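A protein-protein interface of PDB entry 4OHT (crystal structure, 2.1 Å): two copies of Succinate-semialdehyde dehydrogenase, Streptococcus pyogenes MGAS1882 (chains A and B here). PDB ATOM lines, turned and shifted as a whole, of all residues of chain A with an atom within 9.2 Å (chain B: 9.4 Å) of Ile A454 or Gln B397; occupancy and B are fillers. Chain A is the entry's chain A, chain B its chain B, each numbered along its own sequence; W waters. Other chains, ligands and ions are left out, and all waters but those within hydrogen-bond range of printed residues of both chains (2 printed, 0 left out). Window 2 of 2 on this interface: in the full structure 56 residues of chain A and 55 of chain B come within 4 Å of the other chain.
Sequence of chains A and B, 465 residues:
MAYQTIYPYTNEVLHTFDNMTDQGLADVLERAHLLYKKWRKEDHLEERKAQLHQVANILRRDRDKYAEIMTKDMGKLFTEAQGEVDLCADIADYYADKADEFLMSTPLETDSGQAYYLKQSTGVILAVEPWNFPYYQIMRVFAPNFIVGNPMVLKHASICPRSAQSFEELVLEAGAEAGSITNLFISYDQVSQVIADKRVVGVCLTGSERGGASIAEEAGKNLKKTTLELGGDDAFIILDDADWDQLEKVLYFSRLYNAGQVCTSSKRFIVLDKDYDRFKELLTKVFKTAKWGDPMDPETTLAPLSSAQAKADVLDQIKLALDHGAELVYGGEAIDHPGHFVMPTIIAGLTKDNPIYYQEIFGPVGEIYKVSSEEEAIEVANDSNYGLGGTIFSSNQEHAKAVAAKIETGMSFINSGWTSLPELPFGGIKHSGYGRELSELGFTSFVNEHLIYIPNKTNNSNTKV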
ATOM      1  N   THR A 110      13.925 -19.546  -6.776  1.00  0.00           N
ATOM      2  CA  THR A 110      13.256 -20.051  -7.966  1.00  0.00           C
ATOM      3  C   THR A 110      11.954 -19.285  -8.146  1.00  0.00           C
ATOM      4  O   THR A 110      11.265 -18.984  -7.170  1.00  0.00           O
ATOM      5  CB  THR A 110      12.925 -21.556  -7.845  1.00  0.00           C
ATOM      6  OG1 THR A 110      12.265 -21.997  -9.039  1.00  0.00           O
ATOM      7  CG2 THR A 110      12.008 -21.812  -6.649  1.00  0.00           C
ATOM      8  N   ASP A 111      11.618 -18.962  -9.391  1.00  0.00           N
ATOM      9  CA  ASP A 111      10.383 -18.238  -9.657  1.00  0.00           C
ATOM     10  C   ASP A 111       9.292 -19.195 -10.124  1.00  0.00           C
ATOM     11  O   ASP A 111       8.236 -18.765 -10.578  1.00  0.00           O
ATOM     12  CB  ASP A 111      10.613 -17.145 -10.710  1.00  0.00           C
ATOM     13  CG  ASP A 111      11.152 -17.697 -12.015  1.00  0.00           C
ATOM     14  OD1 ASP A 111      10.518 -18.615 -12.581  1.00  0.00           O
ATOM     15  OD2 ASP A 111      12.208 -17.207 -12.477  1.00  0.00           O
ATOM     16  N   SER A 112       9.543 -20.496  -9.997  1.00  0.00           N
ATOM     17  CA  SER A 112       8.569 -21.497 -10.417  1.00  0.00           C
ATOM     18  C   SER A 112       7.762 -22.054  -9.242  1.00  0.00           C
ATOM     19  O   SER A 112       6.768 -22.752  -9.442  1.00  0.00           O
ATOM     20  CB  SER A 112       9.273 -22.648 -11.142  1.00  0.00           C
ATOM     21  OG  SER A 112      10.062 -23.406 -10.240  1.00  0.00           O
ATOM     22  N   GLY A 113       8.190 -21.742  -8.021  1.00  0.00           N
ATOM     23  CA  GLY A 113       7.480 -22.224  -6.847  1.00  0.00           C
ATOM     24  C   GLY A 113       8.253 -22.031  -5.553  1.00  0.00           C
ATOM     25  O   GLY A 113       9.178 -21.217  -5.487  1.00  0.00           O
ATOM     26  N   GLN A 114       7.867 -22.774  -4.516  1.00  0.00           N
ATOM     27  CA  GLN A 114       8.534 -22.697  -3.220  1.00  0.00           C
ATOM     28  C   GLN A 114       9.524 -23.856  -3.109  1.00  0.00           C
ATOM     29  O   GLN A 114       9.155 -25.015  -3.316  1.00  0.00           O
ATOM     30  CB  GLN A 114       7.507 -22.785  -2.087  1.00  0.00           C
ATOM     31  CG  GLN A 114       8.118 -23.129  -0.719  1.00  0.00           C
ATOM     32  CD  GLN A 114       7.087 -23.196   0.403  1.00  0.00           C
ATOM     33  OE1 GLN A 114       7.369 -23.702   1.496  1.00  0.00           O
ATOM     34  NE2 GLN A 114       5.890 -22.678   0.141  1.00  0.00           N
ATOM     35  N   ALA A 115      10.775 -23.550  -2.779  1.00  0.00           N
ATOM     36  CA  ALA A 115      11.785 -24.594  -2.665  1.00  0.00           C
ATOM     37  C   ALA A 115      12.832 -24.353  -1.586  1.00  0.00           C
ATOM     38  O   ALA A 115      13.285 -23.228  -1.364  1.00  0.00           O
ATOM     39  CB  ALA A 115      12.473 -24.787  -4.004  1.00  0.00           C
ATOM     40  N   TYR A 116      13.216 -25.436  -0.920  1.00  0.00           N
ATOM     41  CA  TYR A 116      14.233 -25.385   0.117  1.00  0.00           C
ATOM     42  C   TYR A 116      14.680 -26.814   0.390  1.00  0.00           C
ATOM     43  O   TYR A 116      14.066 -27.757  -0.100  1.00  0.00           O
ATOM     44  CB  TYR A 116      13.668 -24.760   1.398  1.00  0.00           C
ATOM     45  CG  TYR A 116      12.581 -25.576   2.053  1.00  0.00           C
ATOM     46  CD1 TYR A 116      12.888 -26.563   2.995  1.00  0.00           C
ATOM     47  CD2 TYR A 116      11.243 -25.378   1.714  1.00  0.00           C
ATOM     48  CE1 TYR A 116      11.882 -27.333   3.585  1.00  0.00           C
ATOM     49  CE2 TYR A 116      10.235 -26.136   2.290  1.00  0.00           C
ATOM     50  CZ  TYR A 116      10.558 -27.111   3.224  1.00  0.00           C
ATOM     51  OH  TYR A 116       9.549 -27.857   3.782  1.00  0.00           O
ATOM     52  N   LEU A 451      15.544 -32.080  -0.621  1.00  0.00           N
ATOM     53  CA  LEU A 451      14.807 -31.033  -1.325  1.00  0.00           C
ATOM     54  C   LEU A 451      13.302 -31.168  -1.144  1.00  0.00           C
ATOM     55  O   LEU A 451      12.749 -32.267  -1.214  1.00  0.00           O
ATOM     56  CB  LEU A 451      15.124 -31.066  -2.827  1.00  0.00           C
ATOM     57  CG  LEU A 451      14.209 -30.233  -3.749  1.00  0.00           C
ATOM     58  CD1 LEU A 451      14.510 -28.749  -3.579  1.00  0.00           C
ATOM     59  CD2 LEU A 451      14.409 -30.646  -5.213  1.00  0.00           C
ATOM     60  N   ILE A 452      12.649 -30.039  -0.895  1.00  0.00           N
ATOM     61  CA  ILE A 452      11.201 -29.997  -0.766  1.00  0.00           C
ATOM     62  C   ILE A 452      10.781 -28.977  -1.826  1.00  0.00           C
ATOM     63  O   ILE A 452      11.192 -27.820  -1.769  1.00  0.00           O
ATOM     64  CB  ILE A 452      10.746 -29.482   0.620  1.00  0.00           C
ATOM     65  CG1 ILE A 452      11.310 -30.371   1.737  1.00  0.00           C
ATOM     66  CG2 ILE A 452       9.220 -29.449   0.677  1.00  0.00           C
ATOM     67  CD1 ILE A 452      10.848 -31.807   1.691  1.00  0.00           C
ATOM     68  N   TYR A 453       9.974 -29.401  -2.795  1.00  0.00           N
ATOM     69  CA  TYR A 453       9.551 -28.496  -3.856  1.00  0.00           C
ATOM     70  C   TYR A 453       8.041 -28.430  -4.057  1.00  0.00           C
ATOM     71  O   TYR A 453       7.373 -29.459  -4.178  1.00  0.00           O
ATOM     72  CB  TYR A 453      10.216 -28.900  -5.175  1.00  0.00           C
ATOM     73  CG  TYR A 453       9.856 -28.011  -6.345  1.00  0.00           C
ATOM     74  CD1 TYR A 453      10.192 -26.657  -6.345  1.00  0.00           C
ATOM     75  CD2 TYR A 453       9.180 -28.525  -7.451  1.00  0.00           C
ATOM     76  CE1 TYR A 453       9.864 -25.835  -7.419  1.00  0.00           C
ATOM     77  CE2 TYR A 453       8.845 -27.711  -8.530  1.00  0.00           C
ATOM     78  CZ  TYR A 453       9.190 -26.366  -8.508  1.00  0.00           C
ATOM     79  OH  TYR A 453       8.855 -25.551  -9.564  1.00  0.00           O
ATOM     80  N   ILE A 454       7.513 -27.208  -4.081  1.00  0.00           N
ATOM     81  CA  ILE A 454       6.087 -26.978  -4.298  1.00  0.00           C
ATOM     82  C   ILE A 454       5.936 -26.033  -5.492  1.00  0.00           C
ATOM     83  O   ILE A 454       6.183 -24.834  -5.374  1.00  0.00           O
ATOM     84  CB  ILE A 454       5.415 -26.286  -3.098  1.00  0.00           C
ATOM     85  CG1 ILE A 454       5.674 -27.074  -1.811  1.00  0.00           C
ATOM     86  CG2 ILE A 454       3.916 -26.157  -3.360  1.00  0.00           C
ATOM     87  CD1 ILE A 454       5.154 -26.385  -0.554  1.00  0.00           C
ATOM     88  N   PRO A 455       5.535 -26.559  -6.657  1.00  0.00           N
ATOM     89  CA  PRO A 455       5.380 -25.676  -7.822  1.00  0.00           C
ATOM     90  C   PRO A 455       4.183 -24.740  -7.703  1.00  0.00           C
ATOM     91  O   PRO A 455       3.195 -25.061  -7.044  1.00  0.00           O
ATOM     92  CB  PRO A 455       5.235 -26.658  -8.984  1.00  0.00           C
ATOM     93  CG  PRO A 455       4.576 -27.859  -8.329  1.00  0.00           C
ATOM     94  CD  PRO A 455       5.329 -27.973  -7.019  1.00  0.00           C
ATOM     95  N   ASN A 456       4.276 -23.575  -8.336  1.00  0.00           N
ATOM     96  CA  ASN A 456       3.184 -22.600  -8.309  1.00  0.00           C
ATOM     97  C   ASN A 456       1.954 -23.158  -9.015  1.00  0.00           C
ATOM     98  O   ASN A 456       2.173 -23.868 -10.021  1.00  0.00           O
ATOM     99  CB  ASN A 456       3.608 -21.296  -8.993  1.00  0.00           C
ATOM    100  CG  ASN A 456       4.688 -20.568  -8.232  1.00  0.00           C
ATOM    101  OD1 ASN A 456       4.674 -20.534  -7.005  1.00  0.00           O
ATOM    102  ND2 ASN A 456       5.625 -19.966  -8.954  1.00  0.00           N
ATOM    103  N   LEU B 239      -2.604 -38.270   0.657  1.00  0.00           N
ATOM    104  CA  LEU B 239      -3.160 -38.067   1.987  1.00  0.00           C
ATOM    105  C   LEU B 239      -4.670 -37.870   1.981  1.00  0.00           C
ATOM    106  O   LEU B 239      -5.300 -37.802   0.922  1.00  0.00           O
ATOM    107  CB  LEU B 239      -2.476 -36.875   2.663  1.00  0.00           C
ATOM    108  CG  LEU B 239      -0.944 -36.927   2.709  1.00  0.00           C
ATOM    109  CD1 LEU B 239      -0.438 -35.830   3.622  1.00  0.00           C
ATOM    110  CD2 LEU B 239      -0.470 -38.286   3.214  1.00  0.00           C
ATOM    111  N   ASP B 241      -6.546 -35.244   2.730  1.00  0.00           N
ATOM    112  CA  ASP B 241      -7.070 -34.008   2.151  1.00  0.00           C
ATOM    113  C   ASP B 241      -6.546 -33.709   0.745  1.00  0.00           C
ATOM    114  O   ASP B 241      -6.367 -32.548   0.374  1.00  0.00           O
ATOM    115  CB  ASP B 241      -6.781 -32.818   3.071  1.00  0.00           C
ATOM    116  CG  ASP B 241      -5.346 -32.776   3.538  1.00  0.00           C
ATOM    117  OD1 ASP B 241      -4.474 -33.376   2.867  1.00  0.00           O
ATOM    118  OD2 ASP B 241      -5.085 -32.132   4.577  1.00  0.00           O
ATOM    119  N   GLN B 246      -6.932 -32.007  -8.974  1.00  0.00           N
ATOM    120  CA  GLN B 246      -5.543 -31.699  -9.271  1.00  0.00           C
ATOM    121  C   GLN B 246      -4.789 -33.013  -9.494  1.00  0.00           C
ATOM    122  O   GLN B 246      -3.913 -33.102 -10.356  1.00  0.00           O
ATOM    123  CB  GLN B 246      -4.941 -30.908  -8.105  1.00  0.00           C
ATOM    124  CG  GLN B 246      -3.449 -30.605  -8.215  1.00  0.00           C
ATOM    125  CD  GLN B 246      -2.986 -29.565  -7.192  1.00  0.00           C
ATOM    126  OE1 GLN B 246      -3.407 -29.583  -6.030  1.00  0.00           O
ATOM    127  NE2 GLN B 246      -2.110 -28.660  -7.619  1.00  0.00           N
ATOM    128  N   ILE B 392       4.137 -36.015  -2.243  1.00  0.00           N
ATOM    129  CA  ILE B 392       3.150 -35.954  -1.178  1.00  0.00           C
ATOM    130  C   ILE B 392       1.989 -35.139  -1.752  1.00  0.00           C
ATOM    131  O   ILE B 392       2.165 -33.986  -2.153  1.00  0.00           O
ATOM    132  CB  ILE B 392       3.679 -35.248   0.097  1.00  0.00           C
ATOM    133  CG1 ILE B 392       4.968 -35.919   0.592  1.00  0.00           C
ATOM    134  CG2 ILE B 392       2.627 -35.339   1.195  1.00  0.00           C
ATOM    135  CD1 ILE B 392       4.783 -37.354   1.039  1.00  0.00           C
ATOM    136  N   PHE B 393       0.809 -35.741  -1.806  1.00  0.00           N
ATOM    137  CA  PHE B 393      -0.366 -35.056  -2.337  1.00  0.00           C
ATOM    138  C   PHE B 393      -1.312 -34.669  -1.203  1.00  0.00           C
ATOM    139  O   PHE B 393      -1.887 -35.529  -0.536  1.00  0.00           O
ATOM    140  CB  PHE B 393      -1.069 -35.951  -3.352  1.00  0.00           C
ATOM    141  CG  PHE B 393      -1.417 -35.248  -4.628  1.00  0.00           C
ATOM    142  CD1 PHE B 393      -2.603 -34.524  -4.740  1.00  0.00           C
ATOM    143  CD2 PHE B 393      -0.543 -35.278  -5.712  1.00  0.00           C
ATOM    144  CE1 PHE B 393      -2.918 -33.834  -5.921  1.00  0.00           C
ATOM    145  CE2 PHE B 393      -0.842 -34.596  -6.894  1.00  0.00           C
ATOM    146  CZ  PHE B 393      -2.035 -33.871  -6.998  1.00  0.00           C
ATOM    147  N   SER B 394      -1.461 -33.363  -0.996  1.00  0.00           N
ATOM    148  CA  SER B 394      -2.303 -32.837   0.074  1.00  0.00           C
ATOM    149  C   SER B 394      -2.654 -31.368  -0.180  1.00  0.00           C
ATOM    150  O   SER B 394      -1.790 -30.572  -0.551  1.00  0.00           O
ATOM    151  CB  SER B 394      -1.556 -32.967   1.410  1.00  0.00           C
ATOM    152  OG  SER B 394      -2.211 -32.274   2.457  1.00  0.00           O
ATOM    153  N   SER B 395      -3.918 -31.014   0.026  1.00  0.00           N
ATOM    154  CA  SER B 395      -4.369 -29.637  -0.177  1.00  0.00           C
ATOM    155  C   SER B 395      -3.789 -28.698   0.874  1.00  0.00           C
ATOM    156  O   SER B 395      -3.731 -27.489   0.675  1.00  0.00           O
ATOM    157  CB  SER B 395      -5.893 -29.562  -0.124  1.00  0.00           C
ATOM    158  OG  SER B 395      -6.458 -30.280  -1.204  1.00  0.00           O
ATOM    159  N   ASN B 396      -3.372 -29.265   1.998  1.00  0.00           N
ATOM    160  CA  ASN B 396      -2.789 -28.485   3.083  1.00  0.00           C
ATOM    161  C   ASN B 396      -1.273 -28.569   2.918  1.00  0.00           C
ATOM    162  O   ASN B 396      -0.652 -29.590   3.241  1.00  0.00           O
ATOM    163  CB  ASN B 396      -3.217 -29.081   4.425  1.00  0.00           C
ATOM    164  CG  ASN B 396      -2.797 -28.231   5.606  1.00  0.00           C
ATOM    165  OD1 ASN B 396      -1.690 -27.696   5.642  1.00  0.00           O
ATOM    166  ND2 ASN B 396      -3.680 -28.119   6.593  1.00  0.00           N
ATOM    167  N   GLN B 397      -0.679 -27.497   2.408  1.00  0.00           N
ATOM    168  CA  GLN B 397       0.759 -27.472   2.174  1.00  0.00           C
ATOM    169  C   GLN B 397       1.606 -27.677   3.421  1.00  0.00           C
ATOM    170  O   GLN B 397       2.632 -28.361   3.376  1.00  0.00           O
ATOM    171  CB  GLN B 397       1.143 -26.176   1.460  1.00  0.00           C
ATOM    172  CG  GLN B 397       0.940 -26.278  -0.045  1.00  0.00           C
ATOM    173  CD  GLN B 397       1.107 -24.955  -0.764  1.00  0.00           C
ATOM    174  OE1 GLN B 397       1.911 -24.111  -0.362  1.00  0.00           O
ATOM    175  NE2 GLN B 397       0.358 -24.775  -1.848  1.00  0.00           N
ATOM    176  N   GLU B 398       1.175 -27.099   4.534  1.00  0.00           N
ATOM    177  CA  GLU B 398       1.902 -27.239   5.787  1.00  0.00           C
ATOM    178  C   GLU B 398       1.941 -28.727   6.161  1.00  0.00           C
ATOM    179  O   GLU B 398       2.985 -29.270   6.520  1.00  0.00           O
ATOM    180  CB  GLU B 398       1.198 -26.413   6.869  1.00  0.00           C
ATOM    181  CG  GLU B 398       1.881 -26.404   8.200  1.00  0.00           C
ATOM    182  CD  GLU B 398       1.109 -25.599   9.234  1.00  0.00           C
ATOM    183  OE1 GLU B 398       1.207 -24.353   9.234  1.00  0.00           O
ATOM    184  OE2 GLU B 398       0.389 -26.216  10.045  1.00  0.00           O
ATOM    185  N   HIS B 399       0.796 -29.384   6.041  1.00  0.00           N
ATOM    186  CA  HIS B 399       0.690 -30.805   6.338  1.00  0.00           C
ATOM    187  C   HIS B 399       1.563 -31.652   5.393  1.00  0.00           C
ATOM    188  O   HIS B 399       2.250 -32.583   5.828  1.00  0.00           O
ATOM    189  CB  HIS B 399      -0.767 -31.251   6.203  1.00  0.00           C
ATOM    190  CG  HIS B 399      -1.000 -32.673   6.603  1.00  0.00           C
ATOM    191  ND1 HIS B 399      -1.966 -33.464   6.016  1.00  0.00           N
ATOM    192  CD2 HIS B 399      -0.397 -33.445   7.540  1.00  0.00           C
ATOM    193  CE1 HIS B 399      -1.946 -34.662   6.573  1.00  0.00           C
ATOM    194  NE2 HIS B 399      -1.004 -34.677   7.500  1.00  0.00           N
ATOM    195  N   ALA B 400       1.531 -31.330   4.103  1.00  0.00           N
ATOM    196  CA  ALA B 400       2.319 -32.071   3.119  1.00  0.00           C
ATOM    197  C   ALA B 400       3.810 -31.958   3.431  1.00  0.00           C
ATOM    198  O   ALA B 400       4.552 -32.935   3.332  1.00  0.00           O
ATOM    199  CB  ALA B 400       2.037 -31.548   1.714  1.00  0.00           C
ATOM    200  N   LYS B 401       4.240 -30.757   3.806  1.00  0.00           N
ATOM    201  CA  LYS B 401       5.638 -30.509   4.135  1.00  0.00           C
ATOM    202  C   LYS B 401       6.066 -31.271   5.389  1.00  0.00           C
ATOM    203  O   LYS B 401       7.190 -31.770   5.465  1.00  0.00           O
ATOM    204  CB  LYS B 401       5.876 -29.002   4.311  1.00  0.00           C
ATOM    205  CG  LYS B 401       5.953 -28.237   2.973  1.00  0.00           C
ATOM    206  CD  LYS B 401       5.573 -26.760   3.107  1.00  0.00           C
ATOM    207  CE  LYS B 401       6.583 -25.974   3.913  1.00  0.00           C
ATOM    208  NZ  LYS B 401       6.161 -24.552   4.064  1.00  0.00           N
ATOM    209  N   ALA B 402       5.172 -31.364   6.368  1.00  0.00           N
ATOM    210  CA  ALA B 402       5.486 -32.073   7.600  1.00  0.00           C
ATOM    211  C   ALA B 402       5.662 -33.556   7.305  1.00  0.00           C
ATOM    212  O   ALA B 402       6.561 -34.194   7.834  1.00  0.00           O
ATOM    213  CB  ALA B 402       4.371 -31.867   8.638  1.00  0.00           C
ATOM    214  N   VAL B 403       4.810 -34.105   6.449  1.00  0.00           N
ATOM    215  CA  VAL B 403       4.914 -35.515   6.110  1.00  0.00           C
ATOM    216  C   VAL B 403       6.172 -35.786   5.278  1.00  0.00           C
ATOM    217  O   VAL B 403       6.882 -36.766   5.513  1.00  0.00           O
ATOM    218  CB  VAL B 403       3.670 -35.998   5.342  1.00  0.00           C
ATOM    219  CG1 VAL B 403       3.857 -37.452   4.898  1.00  0.00           C
ATOM    220  CG2 VAL B 403       2.426 -35.865   6.235  1.00  0.00           C
ATOM    221  N   ALA B 404       6.461 -34.900   4.325  1.00  0.00           N
ATOM    222  CA  ALA B 404       7.638 -35.062   3.470  1.00  0.00           C
ATOM    223  C   ALA B 404       8.933 -35.166   4.276  1.00  0.00           C
ATOM    224  O   ALA B 404       9.824 -35.945   3.938  1.00  0.00           O
ATOM    225  CB  ALA B 404       7.734 -33.902   2.480  1.00  0.00           C
ATOM    226  N   ALA B 405       9.038 -34.375   5.340  1.00  0.00           N
ATOM    227  CA  ALA B 405      10.236 -34.391   6.177  1.00  0.00           C
ATOM    228  C   ALA B 405      10.512 -35.767   6.781  1.00  0.00           C
ATOM    229  O   ALA B 405      11.650 -36.082   7.103  1.00  0.00           O
ATOM    230  CB  ALA B 405      10.111 -33.363   7.296  1.00  0.00           C
ATOM    231  N   SER B 412      11.421 -34.385  -2.349  1.00  0.00           N
ATOM    232  CA  SER B 412       9.986 -34.540  -2.115  1.00  0.00           C
ATOM    233  C   SER B 412       9.235 -33.494  -2.937  1.00  0.00           C
ATOM    234  O   SER B 412       9.453 -32.294  -2.757  1.00  0.00           O
ATOM    235  CB  SER B 412       9.650 -34.357  -0.629  1.00  0.00           C
ATOM    236  OG  SER B 412      10.147 -35.431   0.158  1.00  0.00           O
ATOM    237  N   PHE B 413       8.366 -33.949  -3.835  1.00  0.00           N
ATOM    238  CA  PHE B 413       7.578 -33.050  -4.678  1.00  0.00           C
ATOM    239  C   PHE B 413       6.150 -32.980  -4.143  1.00  0.00           C
ATOM    240  O   PHE B 413       5.484 -34.001  -3.974  1.00  0.00           O
ATOM    241  CB  PHE B 413       7.580 -33.550  -6.126  1.00  0.00           C
ATOM    242  CG  PHE B 413       8.959 -33.697  -6.701  1.00  0.00           C
ATOM    243  CD1 PHE B 413       9.715 -32.575  -7.022  1.00  0.00           C
ATOM    244  CD2 PHE B 413       9.524 -34.960  -6.877  1.00  0.00           C
ATOM    245  CE1 PHE B 413      11.014 -32.708  -7.509  1.00  0.00           C
ATOM    246  CE2 PHE B 413      10.825 -35.104  -7.364  1.00  0.00           C
ATOM    247  CZ  PHE B 413      11.571 -33.976  -7.680  1.00  0.00           C
ATOM    248  N   ILE B 414       5.686 -31.764  -3.878  1.00  0.00           N
ATOM    249  CA  ILE B 414       4.348 -31.557  -3.336  1.00  0.00           C
ATOM    250  C   ILE B 414       3.287 -31.337  -4.426  1.00  0.00           C
ATOM    251  O   ILE B 414       3.439 -30.475  -5.290  1.00  0.00           O
ATOM    252  CB  ILE B 414       4.343 -30.340  -2.374  1.00  0.00           C
ATOM    253  CG1 ILE B 414       5.486 -30.474  -1.357  1.00  0.00           C
ATOM    254  CG2 ILE B 414       3.002 -30.224  -1.669  1.00  0.00           C
ATOM    255  CD1 ILE B 414       5.433 -31.744  -0.504  1.00  0.00           C
ATOM    256  N   ASN B 415       2.222 -32.131  -4.372  1.00  0.00           N
ATOM    257  CA  ASN B 415       1.111 -32.029  -5.311  1.00  0.00           C
ATOM    258  C   ASN B 415       1.552 -32.008  -6.760  1.00  0.00           C
ATOM    259  O   ASN B 415       1.021 -31.248  -7.572  1.00  0.00           O
ATOM    260  CB  ASN B 415       0.279 -30.779  -5.008  1.00  0.00           C
ATOM    261  CG  ASN B 415      -0.423 -30.866  -3.667  1.00  0.00           C
ATOM    262  OD1 ASN B 415      -0.877 -31.939  -3.269  1.00  0.00           O
ATOM    263  ND2 ASN B 415      -0.531 -29.737  -2.971  1.00  0.00           N
ATOM    264  N   SER B 416       2.519 -32.855  -7.084  1.00  0.00           N
ATOM    265  CA  SER B 416       3.027 -32.921  -8.444  1.00  0.00           C
ATOM    266  C   SER B 416       4.028 -34.047  -8.570  1.00  0.00           C
ATOM    267  O   SER B 416       4.568 -34.522  -7.566  1.00  0.00           O
ATOM    268  CB  SER B 416       3.702 -31.600  -8.810  1.00  0.00           C
ATOM    269  OG  SER B 416       4.710 -31.270  -7.867  1.00  0.00           O
ATOM    270  N   GLY B 417       4.256 -34.479  -9.805  1.00  0.00           N
ATOM    271  CA  GLY B 417       5.223 -35.522 -10.057  1.00  0.00           C
ATOM    272  C   GLY B 417       6.574 -34.848 -10.017  1.00  0.00           C
ATOM    273  O   GLY B 417       6.676 -33.689  -9.609  1.00  0.00           O
ATOM    274  N   THR B 419      10.115 -32.979 -11.069  1.00  0.00           N
ATOM    275  CA  THR B 419      10.437 -31.807 -11.852  1.00  0.00           C
ATOM    276  C   THR B 419      11.925 -31.575 -11.626  1.00  0.00           C
ATOM    277  O   THR B 419      12.458 -31.905 -10.563  1.00  0.00           O
ATOM    278  CB  THR B 419       9.602 -30.566 -11.403  1.00  0.00           C
ATOM    279  OG1 THR B 419      10.460 -29.429 -11.259  1.00  0.00           O
ATOM    280  CG2 THR B 419       8.894 -30.834 -10.087  1.00  0.00           C
ATOM    281  N   LEU B 421      14.933 -28.549 -12.310  1.00  0.00           N
ATOM    282  CA  LEU B 421      15.282 -27.200 -12.719  1.00  0.00           C
ATOM    283  C   LEU B 421      16.734 -26.960 -12.343  1.00  0.00           C
ATOM    284  O   LEU B 421      17.259 -27.596 -11.424  1.00  0.00           O
ATOM    285  CB  LEU B 421      14.376 -26.180 -12.023  1.00  0.00           C
ATOM    286  CG  LEU B 421      12.900 -26.227 -12.429  1.00  0.00           C
ATOM    287  CD1 LEU B 421      12.090 -25.313 -11.536  1.00  0.00           C
ATOM    288  CD2 LEU B 421      12.752 -25.820 -13.889  1.00  0.00           C
ATOM    289  N   LEU B 424      17.557 -26.291  -8.684  1.00  0.00           N
ATOM    290  CA  LEU B 424      17.215 -27.315  -7.698  1.00  0.00           C
ATOM    291  C   LEU B 424      18.209 -28.474  -7.663  1.00  0.00           C
ATOM    292  O   LEU B 424      18.533 -29.049  -8.702  1.00  0.00           O
ATOM    293  CB  LEU B 424      15.816 -27.875  -7.980  1.00  0.00           C
ATOM    294  CG  LEU B 424      14.634 -26.905  -8.057  1.00  0.00           C
ATOM    295  CD1 LEU B 424      13.363 -27.679  -8.391  1.00  0.00           C
ATOM    296  CD2 LEU B 424      14.478 -26.172  -6.740  1.00  0.00           C
HETATM  297  O   HOH W   1       4.032 -23.212   2.068  1.00  0.00           O
HETATM  298  O   HOH W   2       9.541 -29.833   5.564  1.00  0.00           O
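The side-chain amide oxygen (OE1) of Gln A114 lies within hydrogen-bond range of the side-chain amino group (NZ) of Lys B401 (3.0 Å).
The backbone carbonyl oxygen of Tyr A453 is in hydrogen-bond range of the backbone NH of Ile B414 (2.9 Å).
The backbone carbonyl oxygen of Leu A451 lies within hydrogen-bond range of the backbone NH of Ser B412 (2.7 Å).
The backbone NH (N) of Tyr A453 lies within hydrogen-bond range of the backbone carbonyl oxygen (O) of Ser B412 (2.9 Å).
N of Gln A114 sits at hydrogen-bond distance from O of Ile A454 (2.8 Å).
The backbone NH (N) of Ile A452 lies within hydrogen-bond range of the backbone carbonyl oxygen (O) of Tyr A116, at 2.8 Å.
OG of Ser A112 is in hydrogen-bond range of OH of Tyr A453 (2.6 Å).
O of Ser A112 lies within hydrogen-bond range of N of Asn A456, 2.8 Å away.
OG of Ser A112 touches CD1 of Leu B421, at 3.1 Å.
Leu B424 touches Ala A115 (CD2 to CB, 3.7 Å).
Lys B401 touches Tyr A116 (CE to OH, 3.5 Å).
Tyr A453 touches Thr B419 (CE2 to CG2, 3.5 Å).
Tyr A453 touches Leu B421 (OH to CD1, 3.8 Å).
CD1 of Tyr A453 touches CD1 of Leu B424, at 3.9 Å.
Ile A454 touches Gln B397.
Ile A454 touches Lys B401.
CG of Pro A455 touches OG of Ser B416, at 3.4 Å.
Gly A113 touches none of the printed residues of chain B.
Of the printed residues of chain B, Gln A114 touches Lys B401 (3.0 Å).
Of the printed residues of chain B, Ala A115 touches Leu B424 (3.7 Å).
Tyr A453 touches just these residues of chain B: Ser B412 (2.9 Å), Phe B413 (3.6 Å), Ile B414 (2.9 Å), Thr B419 (3.5 Å), Leu B421 (3.8 Å) and Leu B424 (3.9 Å).
Ile A454 touches three residues of chain B.
Pro A455 touches just these residues of chain B: Ile B414 and Ser B416.
Asn B396 touches none of the printed residues of chain A.
Of chain A, only Ile A454 (3.97 Å) comes within 4 Å of Gln B397.
No residue of chain A comes within 4 Å of Ala B400.
Of the printed residues of chain A, Ser B416 touches Pro A455.
Printed residues of chain A that touch a printed residue of chain B: Ser A112, Gln A114, Ala A115, Tyr A116, Leu A451, Ile A452, Tyr A453, Ile A454 and Pro A455.
Along chain A the printed residues that touch a printed residue of chain B span positions 112 to 455.
Hydrophobic or aromatic side chains of chain B that line the printed part of chain A: Ala B404, Ile B414, Leu B421 and Leu B424.
Among the printed residues, 18 pairs touch across the chains.
Among the printed residues, no Asp or Glu carboxylate lies within 4 Å of a Lys or Arg side-chain nitrogen of the other chain.
No position is printed for both chains.
Of the 18 pairs that touch across the chains among the printed residues, none has its exchanged pair printed and touching as well.
Water W2 bridges OH of Tyr A116 (2.7 Å) and O of Lys B401 (3.0 Å).
Water W1 lies within hydrogen-bond range of the side-chain amide nitrogen (NE2) of Gln A114, the side-chain amino group (NZ) of Lys B401 and the side-chain amide oxygen (OE1) of Gln B397.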
